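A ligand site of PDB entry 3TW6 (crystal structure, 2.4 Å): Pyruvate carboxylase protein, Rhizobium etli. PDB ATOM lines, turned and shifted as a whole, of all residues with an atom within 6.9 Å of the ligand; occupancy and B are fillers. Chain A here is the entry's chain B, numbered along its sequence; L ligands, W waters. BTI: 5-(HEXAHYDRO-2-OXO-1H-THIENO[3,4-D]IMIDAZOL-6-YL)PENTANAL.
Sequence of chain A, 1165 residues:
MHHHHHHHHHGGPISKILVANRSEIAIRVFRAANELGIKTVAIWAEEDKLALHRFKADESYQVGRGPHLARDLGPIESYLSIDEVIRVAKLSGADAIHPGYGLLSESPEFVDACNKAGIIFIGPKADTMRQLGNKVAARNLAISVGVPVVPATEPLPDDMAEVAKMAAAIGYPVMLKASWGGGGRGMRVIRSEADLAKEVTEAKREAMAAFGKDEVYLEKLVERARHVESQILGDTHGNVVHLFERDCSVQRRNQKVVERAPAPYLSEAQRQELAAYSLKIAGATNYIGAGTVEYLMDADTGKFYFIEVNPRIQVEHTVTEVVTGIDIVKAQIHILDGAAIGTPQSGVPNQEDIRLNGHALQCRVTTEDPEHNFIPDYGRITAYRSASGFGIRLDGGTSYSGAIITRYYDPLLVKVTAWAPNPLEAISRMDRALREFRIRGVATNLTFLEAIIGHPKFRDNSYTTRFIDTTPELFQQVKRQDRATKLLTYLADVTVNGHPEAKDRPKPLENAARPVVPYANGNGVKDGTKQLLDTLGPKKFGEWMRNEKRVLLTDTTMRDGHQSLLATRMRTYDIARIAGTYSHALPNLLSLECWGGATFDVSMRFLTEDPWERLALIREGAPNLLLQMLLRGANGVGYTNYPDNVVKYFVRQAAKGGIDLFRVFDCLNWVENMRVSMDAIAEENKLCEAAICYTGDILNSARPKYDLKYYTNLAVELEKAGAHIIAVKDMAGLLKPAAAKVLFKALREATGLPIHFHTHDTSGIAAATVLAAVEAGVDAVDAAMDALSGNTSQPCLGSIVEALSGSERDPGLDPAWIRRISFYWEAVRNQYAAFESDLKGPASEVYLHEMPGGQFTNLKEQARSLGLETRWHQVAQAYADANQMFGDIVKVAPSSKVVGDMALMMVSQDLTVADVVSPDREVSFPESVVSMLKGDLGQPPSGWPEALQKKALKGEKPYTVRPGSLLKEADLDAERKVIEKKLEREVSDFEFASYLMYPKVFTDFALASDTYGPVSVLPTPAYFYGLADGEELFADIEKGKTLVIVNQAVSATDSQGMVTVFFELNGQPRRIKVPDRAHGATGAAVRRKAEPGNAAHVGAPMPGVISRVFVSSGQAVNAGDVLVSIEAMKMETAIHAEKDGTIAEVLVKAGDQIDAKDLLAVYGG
An oxygen (O11) of the ligand is in hydrogen-bond range of the side-chain amino group of Lys 1130 (2.5 Å). ND2 of Asn 445 sits at hydrogen-bond distance from O11 of the ligand.
OD1 of Asp 410 sits close to S1 of the ligand (3.7 Å). Merely in contact with the ligand: Val 257, Arg 364, Thr 366, Glu 368 and Pro 411. Hydrophobic or aromatic side chains that line the ligand: Val 257 and Pro 411. Eight residues have an atom within 4 Å of the ligand: Val 257, Arg 364, Thr 366, Glu 368, Asp 410, Pro 411, Asn 445 and Lys 1130. The nearest printed residue that does not touch the ligand is Leu 449 (4.1 Å).
The guanidinium group (NH2) of Arg 364 is in hydrogen-bond range of the backbone carbonyl oxygen (O) of Lys 256 (2.7 Å). The side-chain carboxylate (OD2) of Asp 410 sits close to the backbone NH (N) of Leu 412. The side-chain amino group (NZ) of Lys 1130 sits close to the side-chain amide nitrogen (ND2) of Asn 445, 3.3 Å away. NZ of Lys 1130 is in salt-bridge range of OE1 of Glu 368. NH2 of Arg 364 is in salt-bridge range of OE2 of Glu 259 (3.0 Å). OG1 of Thr 366 is in hydrogen-bond range of OE1 of Glu 368 (2.5 Å). N of Thr 366 sits at hydrogen-bond distance from OD1 of Asn 445, 2.9 Å away. The backbone carbonyl oxygen (O) of Arg 364 is in hydrogen-bond range of the side-chain amide nitrogen (ND2) of Asn 445, 3.0 Å away.
Water W1 bridges a nitrogen (N2) of the ligand (3.0 Å) and the side-chain carboxylate of Glu 368 (3.3 Å).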
ATOM      1  N   TYR A 101     -14.114   9.487  25.154  1.00  0.00           N
ATOM      2  CA  TYR A 101     -15.404   8.884  25.356  1.00  0.00           C
ATOM      3  C   TYR A 101     -15.482   7.592  24.601  1.00  0.00           C
ATOM      4  O   TYR A 101     -14.754   7.380  23.596  1.00  0.00           O
ATOM      5  CB  TYR A 101     -16.576   9.800  24.942  1.00  0.00           C
ATOM      6  CG  TYR A 101     -16.628  10.317  23.481  1.00  0.00           C
ATOM      7  CD1 TYR A 101     -16.813   9.439  22.370  1.00  0.00           C
ATOM      8  CD2 TYR A 101     -16.526  11.699  23.213  1.00  0.00           C
ATOM      9  CE1 TYR A 101     -16.874   9.937  21.053  1.00  0.00           C
ATOM     10  CE2 TYR A 101     -16.571  12.181  21.892  1.00  0.00           C
ATOM     11  CZ  TYR A 101     -16.752  11.300  20.840  1.00  0.00           C
ATOM     12  OH  TYR A 101     -16.836  11.832  19.602  1.00  0.00           O
ATOM     13  N   ARG A 252     -32.543   9.377  17.344  1.00  0.00           N
ATOM     14  CA  ARG A 252     -32.957   8.316  16.463  1.00  0.00           C
ATOM     15  C   ARG A 252     -32.850   7.024  17.295  1.00  0.00           C
ATOM     16  O   ARG A 252     -31.741   6.660  17.709  1.00  0.00           O
ATOM     17  CB  ARG A 252     -32.041   8.326  15.221  1.00  0.00           C
ATOM     18  CG  ARG A 252     -32.252   7.268  14.133  1.00  0.00           C
ATOM     19  CD  ARG A 252     -33.699   6.935  13.910  1.00  0.00           C
ATOM     20  NE  ARG A 252     -33.922   5.956  12.856  1.00  0.00           N
ATOM     21  CZ  ARG A 252     -35.064   5.271  12.690  1.00  0.00           C
ATOM     22  NH1 ARG A 252     -36.098   5.454  13.534  1.00  0.00           N
ATOM     23  NH2 ARG A 252     -35.173   4.405  11.694  1.00  0.00           N
ATOM     24  N   GLN A 255     -30.661   7.219  20.413  1.00  0.00           N
ATOM     25  CA  GLN A 255     -29.285   7.660  20.195  1.00  0.00           C
ATOM     26  C   GLN A 255     -29.339   9.173  19.904  1.00  0.00           C
ATOM     27  O   GLN A 255     -30.266   9.656  19.241  1.00  0.00           O
ATOM     28  CB  GLN A 255     -28.625   6.883  19.005  1.00  0.00           C
ATOM     29  N   LYS A 256     -28.346   9.928  20.346  1.00  0.00           N
ATOM     30  CA  LYS A 256     -28.467  11.381  20.296  1.00  0.00           C
ATOM     31  C   LYS A 256     -28.119  11.866  18.926  1.00  0.00           C
ATOM     32  O   LYS A 256     -27.149  11.387  18.328  1.00  0.00           O
ATOM     33  CB  LYS A 256     -27.658  12.073  21.425  1.00  0.00           C
ATOM     34  N   VAL A 257     -28.917  12.761  18.364  1.00  0.00           N
ATOM     35  CA  VAL A 257     -28.587  13.250  17.006  1.00  0.00           C
ATOM     36  C   VAL A 257     -28.234  14.739  16.956  1.00  0.00           C
ATOM     37  O   VAL A 257     -27.231  15.146  16.363  1.00  0.00           O
ATOM     38  CB  VAL A 257     -29.674  12.871  15.985  1.00  0.00           C
ATOM     39  CG1 VAL A 257     -29.349  13.474  14.600  1.00  0.00           C
ATOM     40  CG2 VAL A 257     -29.825  11.345  15.932  1.00  0.00           C
ATOM     41  N   VAL A 258     -29.058  15.561  17.586  1.00  0.00           N
ATOM     42  CA  VAL A 258     -28.798  16.987  17.654  1.00  0.00           C
ATOM     43  C   VAL A 258     -28.885  17.324  19.148  1.00  0.00           C
ATOM     44  O   VAL A 258     -29.810  16.859  19.856  1.00  0.00           O
ATOM     45  CB  VAL A 258     -29.831  17.787  16.810  1.00  0.00           C
ATOM     46  CG1 VAL A 258     -29.660  19.282  16.997  1.00  0.00           C
ATOM     47  CG2 VAL A 258     -29.736  17.401  15.337  1.00  0.00           C
ATOM     48  N   GLU A 259     -27.925  18.123  19.617  1.00  0.00           N
ATOM     49  CA  GLU A 259     -27.846  18.511  21.010  1.00  0.00           C
ATOM     50  C   GLU A 259     -27.713  20.041  21.024  1.00  0.00           C
ATOM     51  O   GLU A 259     -27.126  20.631  20.100  1.00  0.00           O
ATOM     52  CB  GLU A 259     -26.609  17.862  21.696  1.00  0.00           C
ATOM     53  CG  GLU A 259     -26.477  16.331  21.577  1.00  0.00           C
ATOM     54  CD  GLU A 259     -25.782  15.809  20.286  1.00  0.00           C
ATOM     55  OE1 GLU A 259     -24.863  16.444  19.702  1.00  0.00           O
ATOM     56  OE2 GLU A 259     -26.158  14.698  19.843  1.00  0.00           O
ATOM     57  N   CYS A 363     -24.316  19.444  15.283  1.00  0.00           N
ATOM     58  CA  CYS A 363     -24.658  18.452  14.274  1.00  0.00           C
ATOM     59  C   CYS A 363     -23.444  17.622  13.939  1.00  0.00           C
ATOM     60  O   CYS A 363     -22.307  18.134  13.872  1.00  0.00           O
ATOM     61  CB  CYS A 363     -25.097  19.166  12.970  1.00  0.00           C
ATOM     62  SG  CYS A 363     -26.803  19.813  13.017  1.00  0.00           S
ATOM     63  N   ARG A 364     -23.661  16.335  13.683  1.00  0.00           N
ATOM     64  CA  ARG A 364     -22.552  15.535  13.233  1.00  0.00           C
ATOM     65  C   ARG A 364     -22.685  15.115  11.767  1.00  0.00           C
ATOM     66  O   ARG A 364     -23.705  14.508  11.363  1.00  0.00           O
ATOM     67  CB  ARG A 364     -22.305  14.359  14.148  1.00  0.00           C
ATOM     68  CG  ARG A 364     -21.470  14.781  15.351  1.00  0.00           C
ATOM     69  CD  ARG A 364     -21.597  13.776  16.478  1.00  0.00           C
ATOM     70  NE  ARG A 364     -22.983  13.727  16.948  1.00  0.00           N
ATOM     71  CZ  ARG A 364     -23.591  12.665  17.497  1.00  0.00           C
ATOM     72  NH1 ARG A 364     -22.937  11.495  17.664  1.00  0.00           N
ATOM     73  NH2 ARG A 364     -24.883  12.789  17.867  1.00  0.00           N
ATOM     74  N   VAL A 365     -21.653  15.468  10.981  1.00  0.00           N
ATOM     75  CA  VAL A 365     -21.644  15.148   9.563  1.00  0.00           C
ATOM     76  C   VAL A 365     -21.064  13.773   9.407  1.00  0.00           C
ATOM     77  O   VAL A 365     -19.955  13.559   9.884  1.00  0.00           O
ATOM     78  CB  VAL A 365     -20.802  16.142   8.805  1.00  0.00           C
ATOM     79  CG1 VAL A 365     -20.769  15.800   7.313  1.00  0.00           C
ATOM     80  CG2 VAL A 365     -21.350  17.541   9.006  1.00  0.00           C
ATOM     81  N   THR A 366     -21.795  12.857   8.767  1.00  0.00           N
ATOM     82  CA  THR A 366     -21.314  11.438   8.654  1.00  0.00           C
ATOM     83  C   THR A 366     -21.358  10.990   7.200  1.00  0.00           C
ATOM     84  O   THR A 366     -21.890  11.720   6.363  1.00  0.00           O
ATOM     85  CB  THR A 366     -22.179  10.452   9.466  1.00  0.00           C
ATOM     86  OG1 THR A 366     -23.492  10.337   8.871  1.00  0.00           O
ATOM     87  CG2 THR A 366     -22.392  10.948  10.872  1.00  0.00           C
ATOM     88  N   GLU A 368     -23.148   8.505   6.317  1.00  0.00           N
ATOM     89  CA  GLU A 368     -24.428   7.784   6.182  1.00  0.00           C
ATOM     90  C   GLU A 368     -25.326   8.364   5.069  1.00  0.00           C
ATOM     91  O   GLU A 368     -25.766   9.527   5.156  1.00  0.00           O
ATOM     92  CB  GLU A 368     -25.176   7.782   7.500  1.00  0.00           C
ATOM     93  CG  GLU A 368     -24.411   7.052   8.585  1.00  0.00           C
ATOM     94  CD  GLU A 368     -24.820   7.485   9.989  1.00  0.00           C
ATOM     95  OE1 GLU A 368     -24.691   8.718  10.326  1.00  0.00           O
ATOM     96  OE2 GLU A 368     -25.270   6.590  10.760  1.00  0.00           O
ATOM     97  N   PHE A 374     -29.301   5.250   4.532  1.00  0.00           N
ATOM     98  CA  PHE A 374     -28.232   5.728   5.477  1.00  0.00           C
ATOM     99  C   PHE A 374     -27.054   4.792   5.679  1.00  0.00           C
ATOM    100  O   PHE A 374     -26.416   4.838   6.712  1.00  0.00           O
ATOM    101  CB  PHE A 374     -28.786   6.172   6.827  1.00  0.00           C
ATOM    102  CG  PHE A 374     -29.726   7.350   6.706  1.00  0.00           C
ATOM    103  CD1 PHE A 374     -29.330   8.620   7.156  1.00  0.00           C
ATOM    104  CD2 PHE A 374     -31.008   7.206   6.118  1.00  0.00           C
ATOM    105  CE1 PHE A 374     -30.207   9.711   7.044  1.00  0.00           C
ATOM    106  CE2 PHE A 374     -31.882   8.295   6.028  1.00  0.00           C
ATOM    107  CZ  PHE A 374     -31.473   9.539   6.482  1.00  0.00           C
ATOM    108  N   TYR A 409     -15.038   1.658  11.315  1.00  0.00           N
ATOM    109  CA  TYR A 409     -15.416   2.349  12.545  1.00  0.00           C
ATOM    110  C   TYR A 409     -16.734   3.100  12.375  1.00  0.00           C
ATOM    111  O   TYR A 409     -17.508   2.784  11.491  1.00  0.00           O
ATOM    112  CB  TYR A 409     -14.291   3.309  12.996  1.00  0.00           C
ATOM    113  CG  TYR A 409     -12.993   2.605  13.187  1.00  0.00           C
ATOM    114  CD1 TYR A 409     -12.678   2.035  14.419  1.00  0.00           C
ATOM    115  CD2 TYR A 409     -12.064   2.506  12.144  1.00  0.00           C
ATOM    116  CE1 TYR A 409     -11.476   1.365  14.618  1.00  0.00           C
ATOM    117  CE2 TYR A 409     -10.825   1.843  12.339  1.00  0.00           C
ATOM    118  CZ  TYR A 409     -10.541   1.275  13.589  1.00  0.00           C
ATOM    119  OH  TYR A 409      -9.360   0.583  13.837  1.00  0.00           O
ATOM    120  N   ASP A 410     -16.971   4.084  13.220  1.00  0.00           N
ATOM    121  CA  ASP A 410     -18.153   4.886  13.139  1.00  0.00           C
ATOM    122  C   ASP A 410     -18.086   5.742  11.820  1.00  0.00           C
ATOM    123  O   ASP A 410     -17.031   5.813  11.217  1.00  0.00           O
ATOM    124  CB  ASP A 410     -18.261   5.708  14.415  1.00  0.00           C
ATOM    125  CG  ASP A 410     -17.407   6.976  14.395  1.00  0.00           C
ATOM    126  OD1 ASP A 410     -17.649   7.870  15.234  1.00  0.00           O
ATOM    127  OD2 ASP A 410     -16.506   7.122  13.552  1.00  0.00           O
ATOM    128  N   PRO A 411     -19.211   6.313  11.333  1.00  0.00           N
ATOM    129  CA  PRO A 411     -19.080   6.974  10.056  1.00  0.00           C
ATOM    130  C   PRO A 411     -18.917   8.489  10.182  1.00  0.00           C
ATOM    131  O   PRO A 411     -19.356   9.201   9.336  1.00  0.00           O
ATOM    132  CB  PRO A 411     -20.407   6.626   9.376  1.00  0.00           C
ATOM    133  CG  PRO A 411     -21.381   6.712  10.487  1.00  0.00           C
ATOM    134  CD  PRO A 411     -20.638   6.111  11.685  1.00  0.00           C
ATOM    135  N   LEU A 412     -18.266   8.988  11.213  1.00  0.00           N
ATOM    136  CA  LEU A 412     -18.185  10.457  11.435  1.00  0.00           C
ATOM    137  C   LEU A 412     -17.150  11.161  10.564  1.00  0.00           C
ATOM    138  O   LEU A 412     -16.058  10.676  10.431  1.00  0.00           O
ATOM    139  CB  LEU A 412     -17.866  10.743  12.909  1.00  0.00           C
ATOM    140  CG  LEU A 412     -17.671  12.201  13.288  1.00  0.00           C
ATOM    141  CD1 LEU A 412     -19.014  12.948  13.216  1.00  0.00           C
ATOM    142  CD2 LEU A 412     -17.083  12.293  14.668  1.00  0.00           C
ATOM    143  N   ASN A 445     -24.556  12.760   5.088  1.00  0.00           N
ATOM    144  CA  ASN A 445     -25.849  12.966   5.685  1.00  0.00           C
ATOM    145  C   ASN A 445     -26.304  14.429   5.682  1.00  0.00           C
ATOM    146  O   ASN A 445     -27.313  14.766   6.306  1.00  0.00           O
ATOM    147  CB  ASN A 445     -25.878  12.388   7.122  1.00  0.00           C
ATOM    148  CG  ASN A 445     -25.096  13.242   8.124  1.00  0.00           C
ATOM    149  OD1 ASN A 445     -24.253  14.044   7.765  1.00  0.00           O
ATOM    150  ND2 ASN A 445     -25.394  13.053   9.405  1.00  0.00           N
ATOM    151  N   PHE A 448     -30.139  15.489   5.367  1.00  0.00           N
ATOM    152  CA  PHE A 448     -30.970  15.017   6.480  1.00  0.00           C
ATOM    153  C   PHE A 448     -30.885  15.960   7.701  1.00  0.00           C
ATOM    154  O   PHE A 448     -31.932  16.348   8.308  1.00  0.00           O
ATOM    155  CB  PHE A 448     -30.555  13.590   6.832  1.00  0.00           C
ATOM    156  CG  PHE A 448     -31.124  13.106   8.134  1.00  0.00           C
ATOM    157  CD1 PHE A 448     -32.423  12.608   8.196  1.00  0.00           C
ATOM    158  CD2 PHE A 448     -30.356  13.112   9.301  1.00  0.00           C
ATOM    159  CE1 PHE A 448     -32.953  12.143   9.400  1.00  0.00           C
ATOM    160  CE2 PHE A 448     -30.876  12.637  10.507  1.00  0.00           C
ATOM    161  CZ  PHE A 448     -32.188  12.165  10.564  1.00  0.00           C
ATOM    162  N   LEU A 449     -29.640  16.330   8.026  1.00  0.00           N
ATOM    163  CA  LEU A 449     -29.347  17.354   9.041  1.00  0.00           C
ATOM    164  C   LEU A 449     -30.064  18.666   8.731  1.00  0.00           C
ATOM    165  O   LEU A 449     -30.529  19.370   9.643  1.00  0.00           O
ATOM    166  CB  LEU A 449     -27.845  17.608   9.070  1.00  0.00           C
ATOM    167  CG  LEU A 449     -26.923  16.487   9.577  1.00  0.00           C
ATOM    168  CD1 LEU A 449     -25.437  16.893   9.568  1.00  0.00           C
ATOM    169  CD2 LEU A 449     -27.403  16.043  10.964  1.00  0.00           C
ATOM    170  N   GLU A1127     -26.826  -2.757   9.869  1.00  0.00           N
ATOM    171  CA  GLU A1127     -26.715  -1.302   9.982  1.00  0.00           C
ATOM    172  C   GLU A1127     -27.438  -0.640   8.815  1.00  0.00           C
ATOM    173  O   GLU A1127     -27.140  -0.873   7.621  1.00  0.00           O
ATOM    174  CB  GLU A1127     -25.266  -0.849  10.028  1.00  0.00           C
ATOM    175  CG  GLU A1127     -25.019   0.643  10.309  1.00  0.00           C
ATOM    176  CD  GLU A1127     -23.519   1.049  10.280  1.00  0.00           C
ATOM    177  OE1 GLU A1127     -22.667   0.214   9.876  1.00  0.00           O
ATOM    178  OE2 GLU A1127     -23.159   2.203  10.666  1.00  0.00           O
ATOM    179  N   LYS A1130     -29.798   5.030  10.157  1.00  0.00           N
ATOM    180  CA  LYS A1130     -29.156   5.604  11.330  1.00  0.00           C
ATOM    181  C   LYS A1130     -29.331   4.794  12.617  1.00  0.00           C
ATOM    182  O   LYS A1130     -29.447   5.351  13.691  1.00  0.00           O
ATOM    183  CB  LYS A1130     -29.579   7.051  11.525  1.00  0.00           C
ATOM    184  CG  LYS A1130     -28.754   7.979  10.693  1.00  0.00           C
ATOM    185  CD  LYS A1130     -28.842   9.386  11.210  1.00  0.00           C
ATOM    186  CE  LYS A1130     -28.076  10.274  10.254  1.00  0.00           C
ATOM    187  NZ  LYS A1130     -26.610  10.205  10.463  1.00  0.00           N
ATOM    188  N   GLU A1132     -28.815   0.440  14.349  1.00  0.00           N
ATOM    189  CA  GLU A1132     -28.320  -0.924  14.182  1.00  0.00           C
ATOM    190  C   GLU A1132     -29.372  -1.899  14.764  1.00  0.00           C
ATOM    191  O   GLU A1132     -29.941  -1.631  15.824  1.00  0.00           O
ATOM    192  CB  GLU A1132     -26.970  -1.076  14.858  1.00  0.00           C
ATOM    193  CG  GLU A1132     -25.968  -1.844  13.986  1.00  0.00           C
ATOM    194  CD  GLU A1132     -24.534  -1.308  14.107  1.00  0.00           C
ATOM    195  OE1 GLU A1132     -24.091  -0.529  13.218  1.00  0.00           O
ATOM    196  OE2 GLU A1132     -23.858  -1.640  15.091  1.00  0.00           O
HETATM  197  C11 BTI L   1     -26.496  11.433  12.953  1.00  0.00           C
HETATM  198  O11 BTI L   1     -26.804  12.146  12.000  1.00  0.00           O
HETATM  199  C10 BTI L   1     -25.033  11.176  13.281  1.00  0.00           C
HETATM  200  C9  BTI L   1     -24.907  10.577  14.674  1.00  0.00           C
HETATM  201  C8  BTI L   1     -25.162   9.079  14.642  1.00  0.00           C
HETATM  202  C7  BTI L   1     -23.931   8.315  14.146  1.00  0.00           C
HETATM  203  C2  BTI L   1     -23.015   7.978  15.322  1.00  0.00           C
HETATM  204  S1  BTI L   1     -21.331   8.514  15.085  1.00  0.00           S
HETATM  205  C6  BTI L   1     -20.650   7.398  16.294  1.00  0.00           C
HETATM  206  C5  BTI L   1     -21.666   6.265  16.568  1.00  0.00           C
HETATM  207  N3  BTI L   1     -21.243   4.943  16.087  1.00  0.00           N
HETATM  208  C3  BTI L   1     -22.086   4.473  15.125  1.00  0.00           C
HETATM  209  O3  BTI L   1     -22.019   3.332  14.628  1.00  0.00           O
HETATM  210  N2  BTI L   1     -22.989   5.426  14.809  1.00  0.00           N
HETATM  211  C4  BTI L   1     -22.988   6.502  15.807  1.00  0.00           C
HETATM  212  O   HOH W   1     -25.842   5.913  13.977  1.00  0.00           O
